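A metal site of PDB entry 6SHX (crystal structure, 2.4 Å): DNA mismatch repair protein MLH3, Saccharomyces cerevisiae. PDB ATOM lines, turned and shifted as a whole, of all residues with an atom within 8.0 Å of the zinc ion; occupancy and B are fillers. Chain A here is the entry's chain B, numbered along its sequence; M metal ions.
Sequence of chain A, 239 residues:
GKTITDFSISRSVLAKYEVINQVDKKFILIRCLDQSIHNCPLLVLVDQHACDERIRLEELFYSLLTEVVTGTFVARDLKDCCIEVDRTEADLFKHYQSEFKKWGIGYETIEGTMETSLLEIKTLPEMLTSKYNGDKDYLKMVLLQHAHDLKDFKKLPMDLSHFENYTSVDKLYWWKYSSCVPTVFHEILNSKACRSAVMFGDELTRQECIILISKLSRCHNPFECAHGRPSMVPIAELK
The side-chain carboxylate of Glu 53 lies within hydrogen-bond range of the backbone NH of Ala 226. The backbone carbonyl oxygen (O) of Val 198 lies within hydrogen-bond range of a ring nitrogen (ND1) of His 49, at 2.8 Å. SG of Cys 225 sits close to N of His 227, 3.4 Å away.
Residues that only touch the zinc ion: His 227. Within 4 Å of the zinc ion: His 49, Glu 53, Cys 194 and His 227. The nearest printed residue that does not touch the zinc ion is Arg 195 (5.6 Å).
The zinc ion is bound by the side-chain carboxylate (OE1) of Glu 53 (1.9 Å), a ring nitrogen (NE2) of His 49 (2.3 Å) and the side-chain sulfur (SG) of Cys 194 (2.5 Å).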
ATOM      1  N   ASP A  47      23.176 -10.803  -8.369  1.00  0.00           N
ATOM      2  CA  ASP A  47      22.902 -10.470  -6.978  1.00  0.00           C
ATOM      3  C   ASP A  47      24.069  -9.588  -6.497  1.00  0.00           C
ATOM      4  O   ASP A  47      25.210 -10.053  -6.453  1.00  0.00           O
ATOM      5  CB  ASP A  47      22.778 -11.733  -6.126  1.00  0.00           C
ATOM      6  CG  ASP A  47      22.489 -11.478  -4.659  1.00  0.00           C
ATOM      7  OD1 ASP A  47      21.848 -10.447  -4.351  1.00  0.00           O
ATOM      8  OD2 ASP A  47      22.888 -12.314  -3.813  1.00  0.00           O
ATOM      9  N   HIS A  49      24.893  -8.460  -3.573  1.00  0.00           N
ATOM     10  CA  HIS A  49      25.531  -8.990  -2.378  1.00  0.00           C
ATOM     11  C   HIS A  49      26.531 -10.105  -2.745  1.00  0.00           C
ATOM     12  O   HIS A  49      27.718  -9.994  -2.404  1.00  0.00           O
ATOM     13  CB  HIS A  49      24.508  -9.449  -1.334  1.00  0.00           C
ATOM     14  CG  HIS A  49      25.168 -10.089  -0.154  1.00  0.00           C
ATOM     15  ND1 HIS A  49      25.801  -9.333   0.810  1.00  0.00           N
ATOM     16  CD2 HIS A  49      25.358 -11.398   0.126  1.00  0.00           C
ATOM     17  CE1 HIS A  49      26.330 -10.204   1.654  1.00  0.00           C
ATOM     18  NE2 HIS A  49      26.093 -11.457   1.273  1.00  0.00           N
ATOM     19  N   ALA A  50      26.068 -11.132  -3.497  1.00  0.00           N
ATOM     20  CA  ALA A  50      26.881 -12.251  -3.985  1.00  0.00           C
ATOM     21  C   ALA A  50      28.098 -11.765  -4.779  1.00  0.00           C
ATOM     22  O   ALA A  50      29.208 -12.270  -4.562  1.00  0.00           O
ATOM     23  CB  ALA A  50      26.036 -13.181  -4.839  1.00  0.00           C
ATOM     24  N   GLU A  53      30.587  -9.903  -2.384  1.00  0.00           N
ATOM     25  CA  GLU A  53      31.094 -10.976  -1.517  1.00  0.00           C
ATOM     26  C   GLU A  53      32.192 -11.771  -2.223  1.00  0.00           C
ATOM     27  O   GLU A  53      33.214 -12.067  -1.596  1.00  0.00           O
ATOM     28  CB  GLU A  53      29.937 -11.885  -1.118  1.00  0.00           C
ATOM     29  CG  GLU A  53      30.263 -12.933  -0.080  1.00  0.00           C
ATOM     30  CD  GLU A  53      29.029 -13.727   0.283  1.00  0.00           C
ATOM     31  OE1 GLU A  53      28.246 -13.235   1.126  1.00  0.00           O
ATOM     32  OE2 GLU A  53      28.821 -14.812  -0.301  1.00  0.00           O
ATOM     33  N   ARG A  54      31.990 -12.113  -3.532  1.00  0.00           N
ATOM     34  CA  ARG A  54      32.958 -12.851  -4.356  1.00  0.00           C
ATOM     35  C   ARG A  54      34.234 -12.052  -4.603  1.00  0.00           C
ATOM     36  O   ARG A  54      35.331 -12.636  -4.581  1.00  0.00           O
ATOM     37  CB  ARG A  54      32.357 -13.266  -5.702  1.00  0.00           C
ATOM     38  CG  ARG A  54      33.220 -14.309  -6.434  1.00  0.00           C
ATOM     39  CD  ARG A  54      33.195 -15.608  -5.673  1.00  0.00           C
ATOM     40  NE  ARG A  54      34.417 -16.389  -5.809  1.00  0.00           N
ATOM     41  CZ  ARG A  54      34.515 -17.651  -5.416  1.00  0.00           C
ATOM     42  NH1 ARG A  54      33.458 -18.274  -4.902  1.00  0.00           N
ATOM     43  NH2 ARG A  54      35.650 -18.318  -5.566  1.00  0.00           N
ATOM     44  N   ASN A 190      34.989 -16.600   4.353  1.00  0.00           N
ATOM     45  CA  ASN A 190      33.632 -16.516   3.791  1.00  0.00           C
ATOM     46  C   ASN A 190      32.781 -15.570   4.624  1.00  0.00           C
ATOM     47  O   ASN A 190      32.044 -14.768   4.036  1.00  0.00           O
ATOM     48  CB  ASN A 190      32.960 -17.896   3.788  1.00  0.00           C
ATOM     49  CG  ASN A 190      33.407 -18.874   2.742  1.00  0.00           C
ATOM     50  OD1 ASN A 190      34.047 -18.537   1.744  1.00  0.00           O
ATOM     51  ND2 ASN A 190      33.060 -20.137   2.950  1.00  0.00           N
ATOM     52  N   SER A 191      32.861 -15.662   5.958  1.00  0.00           N
ATOM     53  CA  SER A 191      32.071 -14.837   6.865  1.00  0.00           C
ATOM     54  C   SER A 191      32.513 -13.360   6.876  1.00  0.00           C
ATOM     55  O   SER A 191      31.663 -12.474   6.988  1.00  0.00           O
ATOM     56  CB  SER A 191      32.048 -15.425   8.275  1.00  0.00           C
ATOM     57  OG  SER A 191      33.317 -15.293   8.891  1.00  0.00           O
ATOM     58  N   ALA A 193      34.084 -11.782   4.250  1.00  0.00           N
ATOM     59  CA  ALA A 193      33.699 -11.271   2.933  1.00  0.00           C
ATOM     60  C   ALA A 193      32.207 -10.985   2.872  1.00  0.00           C
ATOM     61  O   ALA A 193      31.805  -9.935   2.349  1.00  0.00           O
ATOM     62  CB  ALA A 193      34.096 -12.251   1.843  1.00  0.00           C
ATOM     63  N   CYS A 194      31.385 -11.888   3.462  1.00  0.00           N
ATOM     64  CA  CYS A 194      29.928 -11.748   3.547  1.00  0.00           C
ATOM     65  C   CYS A 194      29.519 -10.496   4.315  1.00  0.00           C
ATOM     66  O   CYS A 194      28.701  -9.722   3.820  1.00  0.00           O
ATOM     67  CB  CYS A 194      29.303 -13.007   4.149  1.00  0.00           C
ATOM     68  SG  CYS A 194      27.551 -12.848   4.561  1.00  0.00           S
ATOM     69  N   ARG A 195      30.088 -10.294   5.505  1.00  0.00           N
ATOM     70  CA  ARG A 195      29.801  -9.143   6.369  1.00  0.00           C
ATOM     71  C   ARG A 195      30.286  -7.805   5.836  1.00  0.00           C
ATOM     72  O   ARG A 195      29.721  -6.774   6.199  1.00  0.00           O
ATOM     73  CB  ARG A 195      30.339  -9.382   7.780  1.00  0.00           C
ATOM     74  CG  ARG A 195      29.443 -10.267   8.614  1.00  0.00           C
ATOM     75  CD  ARG A 195      30.130 -10.601   9.918  1.00  0.00           C
ATOM     76  NE  ARG A 195      30.077  -9.487  10.861  1.00  0.00           N
ATOM     77  CZ  ARG A 195      29.487  -9.543  12.050  1.00  0.00           C
ATOM     78  NH1 ARG A 195      28.910 -10.665  12.454  1.00  0.00           N
ATOM     79  NH2 ARG A 195      29.492  -8.485  12.849  1.00  0.00           N
ATOM     80  N   SER A 196      31.341  -7.812   5.004  1.00  0.00           N
ATOM     81  CA  SER A 196      31.920  -6.587   4.434  1.00  0.00           C
ATOM     82  C   SER A 196      31.205  -6.149   3.172  1.00  0.00           C
ATOM     83  O   SER A 196      31.264  -4.976   2.816  1.00  0.00           O
ATOM     84  CB  SER A 196      33.396  -6.802   4.151  1.00  0.00           C
ATOM     85  OG  SER A 196      34.150  -6.718   5.344  1.00  0.00           O
ATOM     86  N   ALA A 197      30.515  -7.093   2.492  1.00  0.00           N
ATOM     87  CA  ALA A 197      29.795  -6.904   1.242  1.00  0.00           C
ATOM     88  C   ALA A 197      28.577  -6.018   1.367  1.00  0.00           C
ATOM     89  O   ALA A 197      28.014  -5.852   2.457  1.00  0.00           O
ATOM     90  CB  ALA A 197      29.400  -8.252   0.661  1.00  0.00           C
ATOM     91  N   VAL A 198      28.149  -5.454   0.229  1.00  0.00           N
ATOM     92  CA  VAL A 198      26.962  -4.618   0.077  1.00  0.00           C
ATOM     93  C   VAL A 198      25.727  -5.527   0.265  1.00  0.00           C
ATOM     94  O   VAL A 198      25.762  -6.688  -0.144  1.00  0.00           O
ATOM     95  CB  VAL A 198      27.020  -3.837  -1.278  1.00  0.00           C
ATOM     96  CG1 VAL A 198      26.748  -4.723  -2.488  1.00  0.00           C
ATOM     97  CG2 VAL A 198      26.107  -2.627  -1.260  1.00  0.00           C
ATOM     98  N   MET A 199      24.687  -5.046   0.951  1.00  0.00           N
ATOM     99  CA  MET A 199      23.497  -5.845   1.231  1.00  0.00           C
ATOM    100  C   MET A 199      22.314  -5.560   0.316  1.00  0.00           C
ATOM    101  O   MET A 199      22.390  -4.665  -0.532  1.00  0.00           O
ATOM    102  CB  MET A 199      23.062  -5.589   2.680  1.00  0.00           C
ATOM    103  CG  MET A 199      23.741  -6.467   3.692  1.00  0.00           C
ATOM    104  SD  MET A 199      23.078  -6.161   5.353  1.00  0.00           S
ATOM    105  CE  MET A 199      21.423  -6.946   5.209  1.00  0.00           C
ATOM    106  N   CYS A 225      28.733 -17.245  -5.022  1.00  0.00           N
ATOM    107  CA  CYS A 225      29.007 -16.422  -3.844  1.00  0.00           C
ATOM    108  C   CYS A 225      30.019 -17.166  -2.957  1.00  0.00           C
ATOM    109  O   CYS A 225      30.599 -18.160  -3.406  1.00  0.00           O
ATOM    110  CB  CYS A 225      27.702 -16.116  -3.106  1.00  0.00           C
ATOM    111  SG  CYS A 225      26.842 -17.580  -2.457  1.00  0.00           S
ATOM    112  N   ALA A 226      30.228 -16.713  -1.701  1.00  0.00           N
ATOM    113  CA  ALA A 226      31.141 -17.391  -0.771  1.00  0.00           C
ATOM    114  C   ALA A 226      30.542 -18.696  -0.202  1.00  0.00           C
ATOM    115  O   ALA A 226      31.280 -19.481   0.387  1.00  0.00           O
ATOM    116  CB  ALA A 226      31.526 -16.449   0.364  1.00  0.00           C
ATOM    117  N   HIS A 227      29.228 -18.945  -0.413  1.00  0.00           N
ATOM    118  CA  HIS A 227      28.544 -20.124   0.121  1.00  0.00           C
ATOM    119  C   HIS A 227      28.006 -21.095  -0.948  1.00  0.00           C
ATOM    120  O   HIS A 227      26.958 -21.719  -0.741  1.00  0.00           O
ATOM    121  CB  HIS A 227      27.440 -19.691   1.091  1.00  0.00           C
ATOM    122  CG  HIS A 227      27.930 -18.758   2.143  1.00  0.00           C
ATOM    123  ND1 HIS A 227      27.921 -17.385   1.951  1.00  0.00           N
ATOM    124  CD2 HIS A 227      28.532 -19.031   3.331  1.00  0.00           C
ATOM    125  CE1 HIS A 227      28.460 -16.872   3.044  1.00  0.00           C
ATOM    126  NE2 HIS A 227      28.847 -17.818   3.901  1.00  0.00           N
HETATM  127 ZN    ZN M   1      26.731 -13.384   2.246  1.00  0.00          ZN
